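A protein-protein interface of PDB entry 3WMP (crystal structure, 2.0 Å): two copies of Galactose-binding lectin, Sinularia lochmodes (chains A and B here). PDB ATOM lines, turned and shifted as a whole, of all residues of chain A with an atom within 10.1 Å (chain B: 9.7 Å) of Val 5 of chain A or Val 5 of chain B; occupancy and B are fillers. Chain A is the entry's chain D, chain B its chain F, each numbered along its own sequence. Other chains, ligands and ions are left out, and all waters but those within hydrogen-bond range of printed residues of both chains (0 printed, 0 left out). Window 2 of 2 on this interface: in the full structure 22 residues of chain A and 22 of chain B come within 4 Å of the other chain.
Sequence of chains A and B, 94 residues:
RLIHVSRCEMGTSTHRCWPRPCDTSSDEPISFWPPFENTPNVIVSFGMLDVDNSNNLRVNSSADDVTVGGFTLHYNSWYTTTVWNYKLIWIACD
His 4 of chain A touches Arg 7 of chain B, but with the chains exchanged Arg 7 of chain A does not touch His 4 of chain B (10.0 Å).
Val 5 of chain A touches its own counterpart, Val 5 of chain B.
Ser 6 of chain B touches its own counterpart, Ser 6 of chain A.
Cys 8 of chain B touches its own counterpart, Cys 8 of chain A.
13 positions are printed for both chains.
Of the printed residues of chain B, His 4 of chain A touches Arg 7 and Pro 34.
Of the printed residues of chain B, Val 5 of chain A touches Val 5 and Ser 6.
Of the printed residues of chain B, Ser 6 of chain A touches Ser 6, Arg 7 and Cys 8.
Printed residues of chain B within 4 Å of Cys 8 of chain A: Cys 8.
Val 5 of chain B touches just one residue of chain A: Val 5.
Of the printed residues of chain A, Cys 8 of chain B touches Ser 6 (2.8 Å) and Cys 8 (3.8 Å).
The nearest residue of chain B that does not touch Val 5 of chain A is Arg 7 of chain B (4.4 Å).
The nearest printed residue of chain B that does not touch His 4 of chain A is Ser 6 of chain B (4.7 Å).
O of Ser 6 of chain B sits at hydrogen-bond distance from N of Ser 6 of chain A (2.8 Å).
OG of Ser 6 of chain A lies within hydrogen-bond range of N of Cys 8 of chain B.
SG of Cys 8 of chain B lies close to SG of Cys 8 of chain A (3.8 Å).
The side-chain hydroxyl (OG) of Ser 6 of chain A is in hydrogen-bond range of the chain-end carboxylate (O) of Asp 94 of chain A, 2.7 Å away.
The side-chain sulfur (SG) of Cys 8 of chain A forms a disulfide with the side-chain sulfur (SG) of Cys 93 of chain A (2.0 Å).
The chain-end carboxylate (O) of Asp 94 of chain B sits at hydrogen-bond distance from the side-chain hydroxyl (OG) of Ser 6 of chain B (2.9 Å).
NE of Arg 7 of chain B is in salt-bridge range of OE2 of Glu 9 of chain B.
The backbone carbonyl oxygen (O) of Pro 34 of chain B is in hydrogen-bond range of the guanidinium group (NH2) of Arg 7 of chain B (2.7 Å).
The side-chain sulfur (SG) of Cys 93 of chain B is disulfide-bonded to the side-chain sulfur (SG) of Cys 8 of chain B, at 2.0 Å.
Of the 15 printed residues of chain B, 5 touch a printed residue of chain A.
Printed residues of chain A that touch a printed residue of chain B: His 4, Val 5, Ser 6 and Cys 8.
Hydrophobic or aromatic side chains of chain A within 4 Å of the printed part of chain B: His 4 and Val 5.
Among the printed residues, no Asp or Glu carboxylate lies within 4 Å of a Lys or Arg side-chain nitrogen of the other chain.
Arg 7 of chain B touches His 4 of chain A.
CG of Pro 34 of chain B touches NE2 of His 4 of chain A, 3.4 Å away.
Val 5 of chain B touches Val 5 of chain A (CG2 to CG1, 3.9 Å).
Val 5 of chain A touches Ser 6 of chain B (C to O, 3.6 Å).
Ser 6 of chain A touches Arg 7 of chain B (OG to CA, 3.6 Å).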
ATOM      1  N   ARG A   1      -3.982  14.203  22.533  1.00  0.00           N
ATOM      2  CA  ARG A   1      -2.513  14.045  22.395  1.00  0.00           C
ATOM      3  C   ARG A   1      -2.151  12.564  22.354  1.00  0.00           C
ATOM      4  O   ARG A   1      -2.931  11.705  22.774  1.00  0.00           O
ATOM      5  CB  ARG A   1      -1.798  14.722  23.575  1.00  0.00           C
ATOM      6  CG  ARG A   1      -1.866  13.953  24.886  1.00  0.00           C
ATOM      7  CD  ARG A   1      -1.068  14.643  25.983  1.00  0.00           C
ATOM      8  NE  ARG A   1      -0.939  13.817  27.180  1.00  0.00           N
ATOM      9  CZ  ARG A   1      -1.925  13.574  28.041  1.00  0.00           C
ATOM     10  NH1 ARG A   1      -3.133  14.096  27.851  1.00  0.00           N
ATOM     11  NH2 ARG A   1      -1.702  12.806  29.102  1.00  0.00           N
ATOM     12  N   LEU A   2      -0.967  12.269  21.829  1.00  0.00           N
ATOM     13  CA  LEU A   2      -0.487  10.897  21.757  1.00  0.00           C
ATOM     14  C   LEU A   2       0.244  10.455  23.023  1.00  0.00           C
ATOM     15  O   LEU A   2       1.115  11.166  23.536  1.00  0.00           O
ATOM     16  CB  LEU A   2       0.472  10.721  20.559  1.00  0.00           C
ATOM     17  CG  LEU A   2      -0.226  10.619  19.195  1.00  0.00           C
ATOM     18  CD1 LEU A   2       0.788  10.617  18.058  1.00  0.00           C
ATOM     19  CD2 LEU A   2      -1.077   9.351  19.159  1.00  0.00           C
ATOM     20  N   ILE A   3      -0.144   9.300  23.553  1.00  0.00           N
ATOM     21  CA  ILE A   3       0.564   8.736  24.693  1.00  0.00           C
ATOM     22  C   ILE A   3       0.851   7.251  24.469  1.00  0.00           C
ATOM     23  O   ILE A   3       0.178   6.591  23.673  1.00  0.00           O
ATOM     24  CB  ILE A   3      -0.223   8.835  26.016  1.00  0.00           C
ATOM     25  CG1 ILE A   3      -1.598   8.199  25.850  1.00  0.00           C
ATOM     26  CG2 ILE A   3      -0.317  10.285  26.454  1.00  0.00           C
ATOM     27  CD1 ILE A   3      -2.347   8.040  27.152  1.00  0.00           C
ATOM     28  N   HIS A   4       1.867   6.750  25.170  1.00  0.00           N
ATOM     29  CA  HIS A   4       2.212   5.338  25.139  1.00  0.00           C
ATOM     30  C   HIS A   4       1.579   4.627  26.340  1.00  0.00           C
ATOM     31  O   HIS A   4       1.833   4.984  27.491  1.00  0.00           O
ATOM     32  CB  HIS A   4       3.730   5.141  25.211  1.00  0.00           C
ATOM     33  CG  HIS A   4       4.413   5.249  23.884  1.00  0.00           C
ATOM     34  ND1 HIS A   4       4.539   4.178  23.022  1.00  0.00           N
ATOM     35  CD2 HIS A   4       5.001   6.302  23.265  1.00  0.00           C
ATOM     36  CE1 HIS A   4       5.178   4.567  21.932  1.00  0.00           C
ATOM     37  NE2 HIS A   4       5.471   5.852  22.054  1.00  0.00           N
ATOM     38  N   VAL A   5       0.728   3.646  26.070  1.00  0.00           N
ATOM     39  CA  VAL A   5       0.143   2.860  27.142  1.00  0.00           C
ATOM     40  C   VAL A   5       0.177   1.390  26.762  1.00  0.00           C
ATOM     41  O   VAL A   5       0.274   1.043  25.587  1.00  0.00           O
ATOM     42  CB  VAL A   5      -1.329   3.234  27.442  1.00  0.00           C
ATOM     43  CG1 VAL A   5      -1.407   4.645  27.993  1.00  0.00           C
ATOM     44  CG2 VAL A   5      -2.175   3.090  26.191  1.00  0.00           C
ATOM     45  N   SER A   6       0.129   0.530  27.765  1.00  0.00           N
ATOM     46  CA  SER A   6       0.094  -0.872  27.500  1.00  0.00           C
ATOM     47  C   SER A   6      -1.076  -1.560  28.193  1.00  0.00           C
ATOM     48  O   SER A   6      -1.507  -1.152  29.275  1.00  0.00           O
ATOM     49  CB  SER A   6       1.387  -1.569  28.016  1.00  0.00           C
ATOM     50  OG  SER A   6       2.516  -1.210  27.244  1.00  0.00           O
ATOM     51  N   ARG A   7      -1.629  -2.539  27.482  1.00  0.00           N
ATOM     52  CA  ARG A   7      -2.538  -3.465  28.128  1.00  0.00           C
ATOM     53  C   ARG A   7      -1.658  -4.748  28.353  1.00  0.00           C
ATOM     54  O   ARG A   7      -0.894  -5.162  27.478  1.00  0.00           O
ATOM     55  CB  ARG A   7      -3.714  -3.843  27.257  1.00  0.00           C
ATOM     56  CG  ARG A   7      -4.547  -4.982  27.803  1.00  0.00           C
ATOM     57  CD  ARG A   7      -5.368  -5.553  26.672  1.00  0.00           C
ATOM     58  NE  ARG A   7      -5.995  -6.820  27.009  1.00  0.00           N
ATOM     59  CZ  ARG A   7      -6.638  -7.573  26.123  1.00  0.00           C
ATOM     60  NH1 ARG A   7      -6.730  -7.168  24.863  1.00  0.00           N
ATOM     61  NH2 ARG A   7      -7.180  -8.729  26.491  1.00  0.00           N
ATOM     62  N   CYS A   8      -1.769  -5.352  29.537  1.00  0.00           N
ATOM     63  CA  CYS A   8      -1.039  -6.572  29.832  1.00  0.00           C
ATOM     64  C   CYS A   8      -1.921  -7.710  30.320  1.00  0.00           C
ATOM     65  O   CYS A   8      -2.867  -7.505  31.075  1.00  0.00           O
ATOM     66  CB  CYS A   8       0.025  -6.347  30.900  1.00  0.00           C
ATOM     67  SG  CYS A   8       1.425  -5.259  30.427  1.00  0.00           S
ATOM     68  N   PHE A  36      -5.933  -8.429  21.471  1.00  0.00           N
ATOM     69  CA  PHE A  36      -5.226  -7.164  21.592  1.00  0.00           C
ATOM     70  C   PHE A  36      -5.506  -6.297  20.350  1.00  0.00           C
ATOM     71  O   PHE A  36      -5.957  -6.796  19.319  1.00  0.00           O
ATOM     72  CB  PHE A  36      -3.707  -7.399  21.660  1.00  0.00           C
ATOM     73  CG  PHE A  36      -3.208  -7.717  23.037  1.00  0.00           C
ATOM     74  CD1 PHE A  36      -3.168  -9.026  23.493  1.00  0.00           C
ATOM     75  CD2 PHE A  36      -2.775  -6.702  23.879  1.00  0.00           C
ATOM     76  CE1 PHE A  36      -2.698  -9.320  24.767  1.00  0.00           C
ATOM     77  CE2 PHE A  36      -2.304  -6.987  25.152  1.00  0.00           C
ATOM     78  CZ  PHE A  36      -2.264  -8.296  25.596  1.00  0.00           C
ATOM     79  N   GLU A  37      -5.264  -4.992  20.473  1.00  0.00           N
ATOM     80  CA  GLU A  37      -5.397  -4.097  19.326  1.00  0.00           C
ATOM     81  C   GLU A  37      -4.128  -4.252  18.475  1.00  0.00           C
ATOM     82  O   GLU A  37      -4.185  -4.228  17.243  1.00  0.00           O
ATOM     83  CB  GLU A  37      -5.544  -2.642  19.770  1.00  0.00           C
ATOM     84  CG  GLU A  37      -6.930  -2.296  20.299  1.00  0.00           C
ATOM     85  CD  GLU A  37      -8.046  -2.875  19.444  1.00  0.00           C
ATOM     86  OE1 GLU A  37      -8.046  -2.640  18.215  1.00  0.00           O
ATOM     87  OE2 GLU A  37      -8.929  -3.565  20.005  1.00  0.00           O
ATOM     88  N   ASN A  38      -2.990  -4.407  19.151  1.00  0.00           N
ATOM     89  CA  ASN A  38      -1.706  -4.611  18.487  1.00  0.00           C
ATOM     90  C   ASN A  38      -1.131  -5.955  18.925  1.00  0.00           C
ATOM     91  O   ASN A  38      -1.417  -6.415  20.028  1.00  0.00           O
ATOM     92  CB  ASN A  38      -0.717  -3.507  18.900  1.00  0.00           C
ATOM     93  CG  ASN A  38      -1.185  -2.123  18.496  1.00  0.00           C
ATOM     94  OD1 ASN A  38      -2.357  -1.918  18.181  1.00  0.00           O
ATOM     95  ND2 ASN A  38      -0.271  -1.163  18.514  1.00  0.00           N
ATOM     96  N   THR A  39      -0.350  -6.603  18.058  1.00  0.00           N
ATOM     97  CA  THR A  39       0.289  -7.863  18.450  1.00  0.00           C
ATOM     98  C   THR A  39       1.152  -7.560  19.677  1.00  0.00           C
ATOM     99  O   THR A  39       2.039  -6.702  19.640  1.00  0.00           O
ATOM    100  CB  THR A  39       1.189  -8.423  17.332  1.00  0.00           C
ATOM    101  OG1 THR A  39       0.439  -8.472  16.108  1.00  0.00           O
ATOM    102  CG2 THR A  39       1.668  -9.836  17.691  1.00  0.00           C
ATOM    103  N   PRO A  40       0.892  -8.254  20.788  1.00  0.00           N
ATOM    104  CA  PRO A  40       1.696  -7.993  21.984  1.00  0.00           C
ATOM    105  C   PRO A  40       3.046  -8.679  21.930  1.00  0.00           C
ATOM    106  O   PRO A  40       3.276  -9.523  21.066  1.00  0.00           O
ATOM    107  CB  PRO A  40       0.846  -8.614  23.102  1.00  0.00           C
ATOM    108  CG  PRO A  40       0.195  -9.798  22.426  1.00  0.00           C
ATOM    109  CD  PRO A  40      -0.091  -9.340  21.005  1.00  0.00           C
ATOM    110  N   ALA A  92       2.138 -10.948  28.567  1.00  0.00           N
ATOM    111  CA  ALA A  92       2.017 -10.354  27.244  1.00  0.00           C
ATOM    112  C   ALA A  92       1.574  -8.905  27.361  1.00  0.00           C
ATOM    113  O   ALA A  92       0.613  -8.616  28.053  1.00  0.00           O
ATOM    114  CB  ALA A  92       0.970 -11.101  26.410  1.00  0.00           C
ATOM    115  N   CYS A  93       2.279  -7.995  26.702  1.00  0.00           N
ATOM    116  CA  CYS A  93       1.845  -6.605  26.689  1.00  0.00           C
ATOM    117  C   CYS A  93       2.001  -6.010  25.289  1.00  0.00           C
ATOM    118  O   CYS A  93       2.896  -6.406  24.547  1.00  0.00           O
ATOM    119  CB  CYS A  93       2.657  -5.737  27.647  1.00  0.00           C
ATOM    120  SG  CYS A  93       2.780  -6.338  29.358  1.00  0.00           S
ATOM    121  N   ASP A  94       1.118  -5.085  24.924  1.00  0.00           N
ATOM    122  CA  ASP A  94       1.270  -4.390  23.654  1.00  0.00           C
ATOM    123  C   ASP A  94       1.757  -2.958  23.936  1.00  0.00           C
ATOM    124  O   ASP A  94       2.365  -2.731  24.991  1.00  0.00           O
ATOM    125  CB  ASP A  94      -0.023  -4.366  22.826  1.00  0.00           C
ATOM    126  CG  ASP A  94      -1.175  -3.633  23.507  1.00  0.00           C
ATOM    127  OD1 ASP A  94      -1.054  -3.178  24.670  1.00  0.00           O
ATOM    128  OD2 ASP A  94      -2.236  -3.516  22.852  1.00  0.00           O
ATOM    129  OXT ASP A  94       1.564  -2.057  23.105  1.00  0.00           O
ATOM    130  N   ARG B   1      -9.005  13.913  34.707  1.00  0.00           N
ATOM    131  CA  ARG B   1      -8.763  13.183  35.973  1.00  0.00           C
ATOM    132  C   ARG B   1      -7.403  12.492  35.957  1.00  0.00           C
ATOM    133  O   ARG B   1      -6.804  12.281  34.900  1.00  0.00           O
ATOM    134  CB  ARG B   1      -9.869  12.143  36.194  1.00  0.00           C
ATOM    135  CG  ARG B   1      -9.700  10.844  35.423  1.00  0.00           C
ATOM    136  CD  ARG B   1     -10.861   9.913  35.716  1.00  0.00           C
ATOM    137  NE  ARG B   1     -10.797   8.644  34.992  1.00  0.00           N
ATOM    138  CZ  ARG B   1     -11.044   8.488  33.691  1.00  0.00           C
ATOM    139  NH1 ARG B   1     -11.383   9.524  32.927  1.00  0.00           N
ATOM    140  NH2 ARG B   1     -10.962   7.278  33.152  1.00  0.00           N
ATOM    141  N   LEU B   2      -6.911  12.161  37.145  1.00  0.00           N
ATOM    142  CA  LEU B   2      -5.647  11.459  37.267  1.00  0.00           C
ATOM    143  C   LEU B   2      -5.857   9.941  37.236  1.00  0.00           C
ATOM    144  O   LEU B   2      -6.710   9.415  37.946  1.00  0.00           O
ATOM    145  CB  LEU B   2      -4.951  11.828  38.590  1.00  0.00           C
ATOM    146  CG  LEU B   2      -4.146  13.140  38.606  1.00  0.00           C
ATOM    147  CD1 LEU B   2      -3.761  13.495  40.032  1.00  0.00           C
ATOM    148  CD2 LEU B   2      -2.903  13.004  37.731  1.00  0.00           C
ATOM    149  N   ILE B   3      -5.119   9.248  36.372  1.00  0.00           N
ATOM    150  CA  ILE B   3      -5.184   7.794  36.360  1.00  0.00           C
ATOM    151  C   ILE B   3      -3.791   7.177  36.262  1.00  0.00           C
ATOM    152  O   ILE B   3      -2.850   7.801  35.757  1.00  0.00           O
ATOM    153  CB  ILE B   3      -6.030   7.213  35.200  1.00  0.00           C
ATOM    154  CG1 ILE B   3      -5.429   7.605  33.855  1.00  0.00           C
ATOM    155  CG2 ILE B   3      -7.461   7.687  35.314  1.00  0.00           C
ATOM    156  CD1 ILE B   3      -6.065   6.882  32.690  1.00  0.00           C
ATOM    157  N   HIS B   4      -3.680   5.946  36.759  1.00  0.00           N
ATOM    158  CA  HIS B   4      -2.444   5.187  36.707  1.00  0.00           C
ATOM    159  C   HIS B   4      -2.404   4.251  35.499  1.00  0.00           C
ATOM    160  O   HIS B   4      -3.217   3.331  35.379  1.00  0.00           O
ATOM    161  CB  HIS B   4      -2.283   4.351  37.979  1.00  0.00           C
ATOM    162  CG  HIS B   4      -1.974   5.163  39.195  1.00  0.00           C
ATOM    163  ND1 HIS B   4      -0.686   5.489  39.567  1.00  0.00           N
ATOM    164  CD2 HIS B   4      -2.786   5.726  40.122  1.00  0.00           C
ATOM    165  CE1 HIS B   4      -0.718   6.216  40.672  1.00  0.00           C
ATOM    166  NE2 HIS B   4      -1.981   6.373  41.029  1.00  0.00           N
ATOM    167  N   VAL B   5      -1.476   4.514  34.587  1.00  0.00           N
ATOM    168  CA  VAL B   5      -1.291   3.633  33.447  1.00  0.00           C
ATOM    169  C   VAL B   5       0.193   3.318  33.315  1.00  0.00           C
ATOM    170  O   VAL B   5       1.044   4.078  33.783  1.00  0.00           O
ATOM    171  CB  VAL B   5      -1.756   4.274  32.114  1.00  0.00           C
ATOM    172  CG1 VAL B   5      -3.219   4.635  32.202  1.00  0.00           C
ATOM    173  CG2 VAL B   5      -0.922   5.499  31.794  1.00  0.00           C
ATOM    174  N   SER B   6       0.490   2.169  32.723  1.00  0.00           N
ATOM    175  CA  SER B   6       1.867   1.829  32.458  1.00  0.00           C
ATOM    176  C   SER B   6       2.080   1.584  30.963  1.00  0.00           C
ATOM    177  O   SER B   6       1.150   1.234  30.233  1.00  0.00           O
ATOM    178  CB  SER B   6       2.283   0.513  33.172  1.00  0.00           C
ATOM    179  OG  SER B   6       2.063   0.589  34.567  1.00  0.00           O
ATOM    180  N   ARG B   7       3.307   1.881  30.542  1.00  0.00           N
ATOM    181  CA  ARG B   7       3.773   1.451  29.235  1.00  0.00           C
ATOM    182  C   ARG B   7       4.816   0.352  29.602  1.00  0.00           C
ATOM    183  O   ARG B   7       5.578   0.511  30.556  1.00  0.00           O
ATOM    184  CB  ARG B   7       4.499   2.544  28.461  1.00  0.00           C
ATOM    185  CG  ARG B   7       5.306   2.056  27.253  1.00  0.00           C
ATOM    186  CD  ARG B   7       6.257   3.151  26.788  1.00  0.00           C
ATOM    187  NE  ARG B   7       7.211   2.683  25.784  1.00  0.00           N
ATOM    188  CZ  ARG B   7       8.263   3.385  25.378  1.00  0.00           C
ATOM    189  NH1 ARG B   7       8.495   4.588  25.892  1.00  0.00           N
ATOM    190  NH2 ARG B   7       9.086   2.885  24.467  1.00  0.00           N
ATOM    191  N   CYS B   8       4.796  -0.770  28.888  1.00  0.00           N
ATOM    192  CA  CYS B   8       5.805  -1.786  29.089  1.00  0.00           C
ATOM    193  C   CYS B   8       6.530  -2.120  27.792  1.00  0.00           C
ATOM    194  O   CYS B   8       5.955  -2.072  26.703  1.00  0.00           O
ATOM    195  CB  CYS B   8       5.221  -3.098  29.617  1.00  0.00           C
ATOM    196  SG  CYS B   8       4.337  -2.976  31.206  1.00  0.00           S
ATOM    197  N   GLU B   9       7.816  -2.410  27.949  1.00  0.00           N
ATOM    198  CA  GLU B   9       8.635  -2.911  26.862  1.00  0.00           C
ATOM    199  C   GLU B   9       9.209  -4.211  27.434  1.00  0.00           C
ATOM    200  O   GLU B   9       9.368  -4.351  28.639  1.00  0.00           O
ATOM    201  CB  GLU B   9       9.792  -1.973  26.483  1.00  0.00           C
ATOM    202  CG  GLU B   9       9.373  -0.575  26.016  1.00  0.00           C
ATOM    203  CD  GLU B   9       8.502  -0.577  24.770  1.00  0.00           C
ATOM    204  OE1 GLU B   9       8.447  -1.620  24.078  1.00  0.00           O
ATOM    205  OE2 GLU B   9       7.877   0.468  24.473  1.00  0.00           O
ATOM    206  N   PRO B  34      10.648   4.775  21.754  1.00  0.00           N
ATOM    207  CA  PRO B  34      11.187   6.006  22.353  1.00  0.00           C
ATOM    208  C   PRO B  34      11.412   5.859  23.849  1.00  0.00           C
ATOM    209  O   PRO B  34      10.917   4.915  24.464  1.00  0.00           O
ATOM    210  CB  PRO B  34      10.099   7.037  22.069  1.00  0.00           C
ATOM    211  CG  PRO B  34       8.844   6.224  22.029  1.00  0.00           C
ATOM    212  CD  PRO B  34       9.237   4.942  21.357  1.00  0.00           C
ATOM    213  N   PHE B  36      11.101   6.255  27.880  1.00  0.00           N
ATOM    214  CA  PHE B  36       9.951   6.346  28.763  1.00  0.00           C
ATOM    215  C   PHE B  36       9.781   7.789  29.259  1.00  0.00           C
ATOM    216  O   PHE B  36      10.726   8.575  29.229  1.00  0.00           O
ATOM    217  CB  PHE B  36      10.152   5.439  29.993  1.00  0.00           C
ATOM    218  CG  PHE B  36       9.901   3.982  29.724  1.00  0.00           C
ATOM    219  CD1 PHE B  36      10.922   3.147  29.285  1.00  0.00           C
ATOM    220  CD2 PHE B  36       8.639   3.441  29.927  1.00  0.00           C
ATOM    221  CE1 PHE B  36      10.687   1.793  29.057  1.00  0.00           C
ATOM    222  CE2 PHE B  36       8.398   2.092  29.702  1.00  0.00           C
ATOM    223  CZ  PHE B  36       9.422   1.265  29.271  1.00  0.00           C
ATOM    224  N   GLU B  37       8.568   8.132  29.691  1.00  0.00           N
ATOM    225  CA  GLU B  37       8.306   9.458  30.256  1.00  0.00           C
ATOM    226  C   GLU B  37       8.889   9.485  31.675  1.00  0.00           C
ATOM    227  O   GLU B  37       9.445  10.497  32.116  1.00  0.00           O
ATOM    228  CB  GLU B  37       6.804   9.740  30.315  1.00  0.00           C
ATOM    229  CG  GLU B  37       6.148   9.874  28.951  1.00  0.00           C
ATOM    230  CD  GLU B  37       6.749  10.992  28.120  1.00  0.00           C
ATOM    231  OE1 GLU B  37       7.075  12.050  28.701  1.00  0.00           O
ATOM    232  OE2 GLU B  37       6.886  10.821  26.889  1.00  0.00           O
ATOM    233  N   ASN B  38       8.738   8.365  32.375  1.00  0.00           N
ATOM    234  CA  ASN B  38       9.276   8.205  33.718  1.00  0.00           C
ATOM    235  C   ASN B  38      10.245   7.021  33.736  1.00  0.00           C
ATOM    236  O   ASN B  38      10.118   6.102  32.933  1.00  0.00           O
ATOM    237  CB  ASN B  38       8.149   7.939  34.724  1.00  0.00           C
ATOM    238  CG  ASN B  38       7.159   9.086  34.807  1.00  0.00           C
ATOM    239  OD1 ASN B  38       7.229  10.046  34.038  1.00  0.00           O
ATOM    240  ND2 ASN B  38       6.225   8.988  35.742  1.00  0.00           N
ATOM    241  N   CYS B  93       8.503  -1.545  32.889  1.00  0.00           N
ATOM    242  CA  CYS B  93       7.257  -0.783  32.871  1.00  0.00           C
ATOM    243  C   CYS B  93       7.381   0.459  33.748  1.00  0.00           C
ATOM    244  O   CYS B  93       8.086   0.444  34.754  1.00  0.00           O
ATOM    245  CB  CYS B  93       6.078  -1.590  33.415  1.00  0.00           C
ATOM    246  SG  CYS B  93       5.770  -3.205  32.640  1.00  0.00           S
ATOM    247  N   ASP B  94       6.711   1.538  33.352  1.00  0.00           N
ATOM    248  CA  ASP B  94       6.708   2.740  34.177  1.00  0.00           C
ATOM    249  C   ASP B  94       5.322   2.915  34.832  1.00  0.00           C
ATOM    250  O   ASP B  94       4.569   1.934  34.956  1.00  0.00           O
ATOM    251  CB  ASP B  94       7.097   3.988  33.368  1.00  0.00           C
ATOM    252  CG  ASP B  94       6.087   4.352  32.283  1.00  0.00           C
ATOM    253  OD1 ASP B  94       5.121   3.595  32.045  1.00  0.00           O
ATOM    254  OD2 ASP B  94       6.271   5.421  31.656  1.00  0.00           O
ATOM    255  OXT ASP B  94       4.972   4.021  35.258  1.00  0.00           O
